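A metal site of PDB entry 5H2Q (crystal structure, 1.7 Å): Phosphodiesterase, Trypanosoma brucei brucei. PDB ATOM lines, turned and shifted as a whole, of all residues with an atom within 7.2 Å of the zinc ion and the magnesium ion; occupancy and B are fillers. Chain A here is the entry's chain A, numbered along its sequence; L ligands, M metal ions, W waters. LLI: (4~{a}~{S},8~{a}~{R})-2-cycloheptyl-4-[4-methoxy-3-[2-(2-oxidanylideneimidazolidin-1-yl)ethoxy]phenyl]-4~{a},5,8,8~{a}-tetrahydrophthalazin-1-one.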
ATOM      1  N   TYR A  87      24.201 -15.083 -13.293  1.00  0.00           N
ATOM      2  CA  TYR A  87      25.166 -14.567 -14.282  1.00  0.00           C
ATOM      3  C   TYR A  87      24.902 -13.140 -14.731  1.00  0.00           C
ATOM      4  O   TYR A  87      25.808 -12.332 -14.674  1.00  0.00           O
ATOM      5  CB  TYR A  87      25.275 -15.499 -15.496  1.00  0.00           C
ATOM      6  CG  TYR A  87      26.320 -15.070 -16.516  1.00  0.00           C
ATOM      7  CD1 TYR A  87      27.667 -15.424 -16.362  1.00  0.00           C
ATOM      8  CD2 TYR A  87      25.989 -14.223 -17.572  1.00  0.00           C
ATOM      9  CE1 TYR A  87      28.624 -15.034 -17.299  1.00  0.00           C
ATOM     10  CE2 TYR A  87      26.950 -13.811 -18.500  1.00  0.00           C
ATOM     11  CZ  TYR A  87      28.266 -14.216 -18.359  1.00  0.00           C
ATOM     12  OH  TYR A  87      29.195 -13.749 -19.266  1.00  0.00           O
ATOM     13  N   HIS A  88      23.673 -12.837 -15.199  1.00  0.00           N
ATOM     14  CA  HIS A  88      23.365 -11.512 -15.709  1.00  0.00           C
ATOM     15  C   HIS A  88      23.015 -10.524 -14.602  1.00  0.00           C
ATOM     16  O   HIS A  88      21.972  -9.871 -14.616  1.00  0.00           O
ATOM     17  CB  HIS A  88      22.298 -11.571 -16.809  1.00  0.00           C
ATOM     18  CG  HIS A  88      22.797 -12.137 -18.111  1.00  0.00           C
ATOM     19  ND1 HIS A  88      22.514 -13.431 -18.484  1.00  0.00           N
ATOM     20  CD2 HIS A  88      23.567 -11.564 -19.061  1.00  0.00           C
ATOM     21  CE1 HIS A  88      23.113 -13.612 -19.649  1.00  0.00           C
ATOM     22  NE2 HIS A  88      23.728 -12.499 -20.062  1.00  0.00           N
ATOM     23  N   HIS A  92      28.461  -8.875 -13.970  1.00  0.00           N
ATOM     24  CA  HIS A  92      28.714  -9.142 -15.382  1.00  0.00           C
ATOM     25  C   HIS A  92      28.993  -7.853 -16.151  1.00  0.00           C
ATOM     26  O   HIS A  92      29.947  -7.797 -16.932  1.00  0.00           O
ATOM     27  CB  HIS A  92      27.511  -9.874 -16.031  1.00  0.00           C
ATOM     28  CG  HIS A  92      27.571  -9.869 -17.529  1.00  0.00           C
ATOM     29  ND1 HIS A  92      28.576 -10.523 -18.216  1.00  0.00           N
ATOM     30  CD2 HIS A  92      26.716  -9.312 -18.416  1.00  0.00           C
ATOM     31  CE1 HIS A  92      28.281 -10.376 -19.499  1.00  0.00           C
ATOM     32  NE2 HIS A  92      27.205  -9.597 -19.666  1.00  0.00           N
ATOM     33  N   VAL A  93      28.143  -6.806 -15.953  1.00  0.00           N
ATOM     34  CA  VAL A  93      28.353  -5.564 -16.716  1.00  0.00           C
ATOM     35  C   VAL A  93      29.610  -4.814 -16.244  1.00  0.00           C
ATOM     36  O   VAL A  93      30.317  -4.216 -17.060  1.00  0.00           O
ATOM     37  CB  VAL A  93      27.102  -4.670 -16.793  1.00  0.00           C
ATOM     38  CG1 VAL A  93      25.947  -5.448 -17.449  1.00  0.00           C
ATOM     39  CG2 VAL A  93      26.691  -4.131 -15.422  1.00  0.00           C
ATOM     40  N   VAL A  96      32.290  -6.610 -18.027  1.00  0.00           N
ATOM     41  CA  VAL A  96      32.333  -6.262 -19.452  1.00  0.00           C
ATOM     42  C   VAL A  96      32.967  -4.878 -19.660  1.00  0.00           C
ATOM     43  O   VAL A  96      33.786  -4.696 -20.576  1.00  0.00           O
ATOM     44  CB  VAL A  96      30.960  -6.428 -20.145  1.00  0.00           C
ATOM     45  CG1 VAL A  96      30.972  -5.816 -21.543  1.00  0.00           C
ATOM     46  CG2 VAL A  96      30.553  -7.907 -20.195  1.00  0.00           C
ATOM     47  N   ALA A 125      28.764  -0.598 -21.923  1.00  0.00           N
ATOM     48  CA  ALA A 125      29.007  -1.861 -21.232  1.00  0.00           C
ATOM     49  C   ALA A 125      28.145  -1.919 -19.966  1.00  0.00           C
ATOM     50  O   ALA A 125      27.619  -2.975 -19.661  1.00  0.00           O
ATOM     51  CB  ALA A 125      30.476  -1.989 -20.860  1.00  0.00           C
ATOM     52  N   HIS A 128      24.240  -2.511 -21.017  1.00  0.00           N
ATOM     53  CA  HIS A 128      23.924  -3.465 -22.066  1.00  0.00           C
ATOM     54  C   HIS A 128      23.037  -4.634 -21.663  1.00  0.00           C
ATOM     55  O   HIS A 128      22.518  -5.289 -22.557  1.00  0.00           O
ATOM     56  CB  HIS A 128      25.182  -3.950 -22.802  1.00  0.00           C
ATOM     57  CG  HIS A 128      25.814  -5.167 -22.218  1.00  0.00           C
ATOM     58  ND1 HIS A 128      26.688  -5.080 -21.171  1.00  0.00           N
ATOM     59  CD2 HIS A 128      25.647  -6.466 -22.559  1.00  0.00           C
ATOM     60  CE1 HIS A 128      27.073  -6.338 -20.926  1.00  0.00           C
ATOM     61  NE2 HIS A 128      26.476  -7.198 -21.735  1.00  0.00           N
ATOM     62  N   ASP A 129      22.854  -4.911 -20.354  1.00  0.00           N
ATOM     63  CA  ASP A 129      21.990  -5.996 -19.915  1.00  0.00           C
ATOM     64  C   ASP A 129      20.983  -5.540 -18.869  1.00  0.00           C
ATOM     65  O   ASP A 129      20.501  -6.388 -18.123  1.00  0.00           O
ATOM     66  CB  ASP A 129      22.835  -7.202 -19.387  1.00  0.00           C
ATOM     67  CG  ASP A 129      23.355  -8.116 -20.491  1.00  0.00           C
ATOM     68  OD1 ASP A 129      22.593  -8.384 -21.444  1.00  0.00           O
ATOM     69  OD2 ASP A 129      24.450  -8.706 -20.308  1.00  0.00           O
ATOM     70  N   LEU A 130      20.603  -4.246 -18.850  1.00  0.00           N
ATOM     71  CA  LEU A 130      19.695  -3.758 -17.807  1.00  0.00           C
ATOM     72  C   LEU A 130      18.404  -4.580 -17.643  1.00  0.00           C
ATOM     73  O   LEU A 130      17.705  -4.866 -18.603  1.00  0.00           O
ATOM     74  CB  LEU A 130      19.296  -2.280 -18.022  1.00  0.00           C
ATOM     75  CG  LEU A 130      20.394  -1.236 -17.886  1.00  0.00           C
ATOM     76  CD1 LEU A 130      20.004   0.028 -18.564  1.00  0.00           C
ATOM     77  CD2 LEU A 130      20.732  -0.926 -16.391  1.00  0.00           C
ATOM     78  N   HIS A 132      17.948  -7.730 -16.891  1.00  0.00           N
ATOM     79  CA  HIS A 132      17.984  -9.144 -17.312  1.00  0.00           C
ATOM     80  C   HIS A 132      17.426  -9.945 -16.138  1.00  0.00           C
ATOM     81  O   HIS A 132      17.657  -9.588 -14.980  1.00  0.00           O
ATOM     82  CB  HIS A 132      19.417  -9.559 -17.633  1.00  0.00           C
ATOM     83  CG  HIS A 132      19.522 -10.694 -18.607  1.00  0.00           C
ATOM     84  ND1 HIS A 132      19.220 -11.996 -18.221  1.00  0.00           N
ATOM     85  CD2 HIS A 132      19.914 -10.696 -19.899  1.00  0.00           C
ATOM     86  CE1 HIS A 132      19.399 -12.737 -19.304  1.00  0.00           C
ATOM     87  NE2 HIS A 132      19.848 -11.993 -20.334  1.00  0.00           N
ATOM     88  N   LEU A 160      15.166  -8.934 -25.409  1.00  0.00           N
ATOM     89  CA  LEU A 160      15.827  -8.302 -24.277  1.00  0.00           C
ATOM     90  C   LEU A 160      16.665  -7.100 -24.670  1.00  0.00           C
ATOM     91  O   LEU A 160      16.742  -6.135 -23.902  1.00  0.00           O
ATOM     92  CB  LEU A 160      16.669  -9.328 -23.535  1.00  0.00           C
ATOM     93  CG  LEU A 160      15.898 -10.415 -22.783  1.00  0.00           C
ATOM     94  CD1 LEU A 160      16.830 -11.543 -22.378  1.00  0.00           C
ATOM     95  CD2 LEU A 160      15.156  -9.838 -21.558  1.00  0.00           C
ATOM     96  N   GLU A 161      17.337  -7.144 -25.813  1.00  0.00           N
ATOM     97  CA  GLU A 161      18.218  -6.028 -26.197  1.00  0.00           C
ATOM     98  C   GLU A 161      17.486  -4.718 -26.413  1.00  0.00           C
ATOM     99  O   GLU A 161      17.970  -3.669 -26.000  1.00  0.00           O
ATOM    100  CB  GLU A 161      19.092  -6.385 -27.405  1.00  0.00           C
ATOM    101  CG  GLU A 161      20.098  -7.508 -27.125  1.00  0.00           C
ATOM    102  CD  GLU A 161      19.503  -8.898 -27.031  1.00  0.00           C
ATOM    103  OE1 GLU A 161      18.383  -9.111 -27.562  1.00  0.00           O
ATOM    104  OE2 GLU A 161      20.170  -9.796 -26.460  1.00  0.00           O
ATOM    105  N   HIS A 164      16.752  -3.510 -22.920  1.00  0.00           N
ATOM    106  CA  HIS A 164      17.948  -2.884 -22.351  1.00  0.00           C
ATOM    107  C   HIS A 164      18.111  -1.469 -22.861  1.00  0.00           C
ATOM    108  O   HIS A 164      18.342  -0.575 -22.058  1.00  0.00           O
ATOM    109  CB  HIS A 164      19.232  -3.720 -22.563  1.00  0.00           C
ATOM    110  CG  HIS A 164      19.132  -5.181 -22.227  1.00  0.00           C
ATOM    111  ND1 HIS A 164      18.506  -5.622 -21.056  1.00  0.00           N
ATOM    112  CD2 HIS A 164      19.682  -6.246 -22.851  1.00  0.00           C
ATOM    113  CE1 HIS A 164      18.619  -6.940 -21.058  1.00  0.00           C
ATOM    114  NE2 HIS A 164      19.323  -7.366 -22.120  1.00  0.00           N
ATOM    115  N   VAL A 199      24.275  -2.014 -28.101  1.00  0.00           N
ATOM    116  CA  VAL A 199      23.408  -2.889 -27.303  1.00  0.00           C
ATOM    117  C   VAL A 199      22.651  -3.855 -28.225  1.00  0.00           C
ATOM    118  O   VAL A 199      22.600  -5.061 -27.940  1.00  0.00           O
ATOM    119  CB  VAL A 199      22.480  -2.128 -26.349  1.00  0.00           C
ATOM    120  CG1 VAL A 199      21.520  -3.073 -25.603  1.00  0.00           C
ATOM    121  CG2 VAL A 199      23.305  -1.296 -25.356  1.00  0.00           C
ATOM    122  N   THR A 202      24.506  -7.023 -29.342  1.00  0.00           N
ATOM    123  CA  THR A 202      24.769  -8.083 -28.379  1.00  0.00           C
ATOM    124  C   THR A 202      23.832  -9.288 -28.494  1.00  0.00           C
ATOM    125  O   THR A 202      24.039 -10.256 -27.761  1.00  0.00           O
ATOM    126  CB  THR A 202      24.825  -7.559 -26.947  1.00  0.00           C
ATOM    127  OG1 THR A 202      23.527  -7.109 -26.606  1.00  0.00           O
ATOM    128  CG2 THR A 202      25.885  -6.470 -26.768  1.00  0.00           C
ATOM    129  N   ASP A 203      22.799  -9.222 -29.356  1.00  0.00           N
ATOM    130  CA  ASP A 203      21.871 -10.340 -29.548  1.00  0.00           C
ATOM    131  C   ASP A 203      22.686 -11.465 -30.261  1.00  0.00           C
ATOM    132  O   ASP A 203      23.041 -11.295 -31.436  1.00  0.00           O
ATOM    133  CB  ASP A 203      20.627  -9.922 -30.365  1.00  0.00           C
ATOM    134  CG  ASP A 203      19.681 -11.083 -30.609  1.00  0.00           C
ATOM    135  OD1 ASP A 203      19.997 -12.195 -30.157  1.00  0.00           O
ATOM    136  OD2 ASP A 203      18.594 -10.844 -31.178  1.00  0.00           O
ATOM    137  N   MET A 204      22.968 -12.571 -29.563  1.00  0.00           N
ATOM    138  CA  MET A 204      23.783 -13.664 -30.132  1.00  0.00           C
ATOM    139  C   MET A 204      23.135 -14.381 -31.340  1.00  0.00           C
ATOM    140  O   MET A 204      23.854 -15.038 -32.108  1.00  0.00           O
ATOM    141  CB  MET A 204      24.221 -14.683 -29.093  1.00  0.00           C
ATOM    142  CG  MET A 204      25.278 -14.182 -28.142  1.00  0.00           C
ATOM    143  SD  MET A 204      26.814 -13.712 -28.984  1.00  0.00           S
ATOM    144  CE  MET A 204      27.492 -15.279 -29.451  1.00  0.00           C
ATOM    145  N   MET A 238      31.980  -4.512 -28.180  1.00  0.00           N
ATOM    146  CA  MET A 238      30.900  -4.799 -27.219  1.00  0.00           C
ATOM    147  C   MET A 238      30.672  -6.319 -27.219  1.00  0.00           C
ATOM    148  O   MET A 238      30.616  -6.958 -26.166  1.00  0.00           O
ATOM    149  CB  MET A 238      29.627  -4.061 -27.674  1.00  0.00           C
ATOM    150  CG  MET A 238      28.495  -4.041 -26.648  1.00  0.00           C
ATOM    151  SD  MET A 238      28.874  -3.511 -24.941  1.00  0.00           S
ATOM    152  CE  MET A 238      29.735  -1.972 -25.205  1.00  0.00           C
ATOM    153  N   GLY A 241      33.596  -8.084 -25.423  1.00  0.00           N
ATOM    154  CA  GLY A 241      33.491  -8.052 -23.970  1.00  0.00           C
ATOM    155  C   GLY A 241      32.453  -9.035 -23.472  1.00  0.00           C
ATOM    156  O   GLY A 241      32.683  -9.741 -22.499  1.00  0.00           O
ATOM    157  N   ASP A 242      31.326  -9.152 -24.205  1.00  0.00           N
ATOM    158  CA  ASP A 242      30.251 -10.081 -23.816  1.00  0.00           C
ATOM    159  C   ASP A 242      30.682 -11.539 -23.819  1.00  0.00           C
ATOM    160  O   ASP A 242      30.236 -12.299 -22.969  1.00  0.00           O
ATOM    161  CB  ASP A 242      29.053  -9.888 -24.727  1.00  0.00           C
ATOM    162  CG  ASP A 242      27.758  -9.590 -24.002  1.00  0.00           C
ATOM    163  OD1 ASP A 242      27.723  -9.736 -22.740  1.00  0.00           O
ATOM    164  OD2 ASP A 242      26.758  -9.332 -24.694  1.00  0.00           O
ATOM    165  N   ILE A 243      31.567 -11.923 -24.760  1.00  0.00           N
ATOM    166  CA  ILE A 243      32.024 -13.310 -24.843  1.00  0.00           C
ATOM    167  C   ILE A 243      33.485 -13.476 -24.360  1.00  0.00           C
ATOM    168  O   ILE A 243      34.140 -14.470 -24.669  1.00  0.00           O
ATOM    169  CB  ILE A 243      31.773 -13.948 -26.226  1.00  0.00           C
ATOM    170  CG1 ILE A 243      32.594 -13.280 -27.369  1.00  0.00           C
ATOM    171  CG2 ILE A 243      30.275 -13.997 -26.544  1.00  0.00           C
ATOM    172  CD1 ILE A 243      32.425 -14.064 -28.783  1.00  0.00           C
HETATM  173  C2  LLI L   1      28.792 -19.397 -22.102  1.00  0.00           C
HETATM  174  C3  LLI L   1      29.552 -18.627 -21.196  1.00  0.00           C
HETATM  175  O1  LLI L   1      29.010 -20.754 -22.059  1.00  0.00           O
HETATM  176  C12 LLI L   1      26.219 -15.298 -23.506  1.00  0.00           C
HETATM  177  C14 LLI L   1      24.693 -15.166 -23.737  1.00  0.00           C
HETATM  178  C15 LLI L   1      24.219 -15.889 -24.991  1.00  0.00           C
HETATM  179  C16 LLI L   1      27.008 -14.564 -24.607  1.00  0.00           C
HETATM  180  C17 LLI L   1      26.431 -13.205 -24.928  1.00  0.00           C
HETATM  181  C18 LLI L   1      24.283 -13.683 -23.752  1.00  0.00           C
HETATM  182  C19 LLI L   1      25.179 -12.861 -24.648  1.00  0.00           C
HETATM  183  C21 LLI L   1      24.611 -17.938 -26.387  1.00  0.00           C
HETATM  184  C22 LLI L   1      24.139 -19.338 -25.849  1.00  0.00           C
HETATM  185  C23 LLI L   1      25.834 -18.015 -27.349  1.00  0.00           C
HETATM  186  C24 LLI L   1      23.705 -20.391 -26.878  1.00  0.00           C
HETATM  187  C25 LLI L   1      25.739 -18.868 -28.606  1.00  0.00           C
HETATM  188  C26 LLI L   1      25.884 -20.380 -28.390  1.00  0.00           C
HETATM  189  C27 LLI L   1      24.837 -21.152 -27.577  1.00  0.00           C
HETATM  190  C28 LLI L   1      28.275 -21.571 -22.990  1.00  0.00           C
HETATM  191  C29 LLI L   1      28.612 -23.007 -22.665  1.00  0.00           C
HETATM  192  C4  LLI L   1      27.822 -18.788 -22.878  1.00  0.00           C
HETATM  193  C5  LLI L   1      29.298 -17.262 -21.070  1.00  0.00           C
HETATM  194  C6  LLI L   1      27.578 -17.418 -22.760  1.00  0.00           C
HETATM  195  C7  LLI L   1      28.314 -16.668 -21.849  1.00  0.00           C
HETATM  196  O8  LLI L   1      30.514 -19.299 -20.498  1.00  0.00           O
HETATM  197  C9  LLI L   1      31.149 -18.636 -19.402  1.00  0.00           C
HETATM  198  C10 LLI L   1      26.522 -16.787 -23.593  1.00  0.00           C
HETATM  199  N11 LLI L   1      25.880 -17.603 -24.405  1.00  0.00           N
HETATM  200  N13 LLI L   1      24.900 -17.078 -25.213  1.00  0.00           N
HETATM  201  O20 LLI L   1      23.339 -15.448 -25.716  1.00  0.00           O
HETATM  202  N30 LLI L   1      27.871 -23.517 -21.501  1.00  0.00           N
HETATM  203  C31 LLI L   1      26.439 -23.266 -21.301  1.00  0.00           C
HETATM  204  C32 LLI L   1      28.460 -23.931 -20.335  1.00  0.00           C
HETATM  205  C33 LLI L   1      26.164 -23.950 -19.962  1.00  0.00           C
HETATM  206  N34 LLI L   1      27.492 -24.176 -19.439  1.00  0.00           N
HETATM  207  O35 LLI L   1      29.662 -24.086 -20.182  1.00  0.00           O
HETATM  208 ZN    ZN M   1      26.066  -9.278 -21.440  1.00  0.00          ZN
HETATM  209 MG    MG M   2      22.597  -9.397 -23.251  1.00  0.00          MG
HETATM  210  O   HOH W   1      24.681  -9.416 -23.252  1.00  0.00           O
HETATM  211  O   HOH W   2      22.533  -7.423 -24.200  1.00  0.00           O
HETATM  212  O   HOH W   3      20.477  -9.442 -23.338  1.00  0.00           O
HETATM  213  O   HOH W   4      25.718 -11.429 -21.595  1.00  0.00           O
HETATM  214  O   HOH W   5      22.649 -11.316 -22.488  1.00  0.00           O
HETATM  215  O   HOH W   6      22.530 -10.161 -25.300  1.00  0.00           O
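Within 4 Å of the magnesium ion: Asp 129.
Water W3 lies within hydrogen-bond range of NE2 of His 164 and OE2 of Glu 161.
Water W6 bridges OE2 of Glu 161 (2.7 Å) and O of Thr 202 (2.9 Å).
Water W2 bridges the side-chain hydroxyl (OG1) of Thr 202 and the backbone carbonyl oxygen (O) of His 128.
Water W5 binds the magnesium ion (2.1 Å).
The magnesium ion is bound by the side-chain carboxylate (OD1) of Asp 129 (2.1 Å).
Water W1 binds the magnesium ion, 2.1 Å away.
Water W3 is bound to the magnesium ion.
The magnesium ion is bound by water W6 (2.2 Å).
Water W2 is bound to the magnesium ion, 2.2 Å away.
The zinc ion is bound by the side-chain carboxylate (OD2) of Asp 129, a ring nitrogen (NE2) of His 92, a ring nitrogen (NE2) of His 128, the side-chain carboxylate (OD1) of Asp 242, water W4 and water W1.
Of the 21 residues printed, 4 come within 4 Å of the zinc ion.
O of Ala 125 lies within hydrogen-bond range of ND1 of His 128 (2.8 Å).
The side-chain carboxylate (OD1) of Asp 129 lies close to a ring nitrogen (NE2) of His 164 (3.5 Å).
ND1 of His 92 sits at hydrogen-bond distance from OH of Tyr 87, 3.4 Å away.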
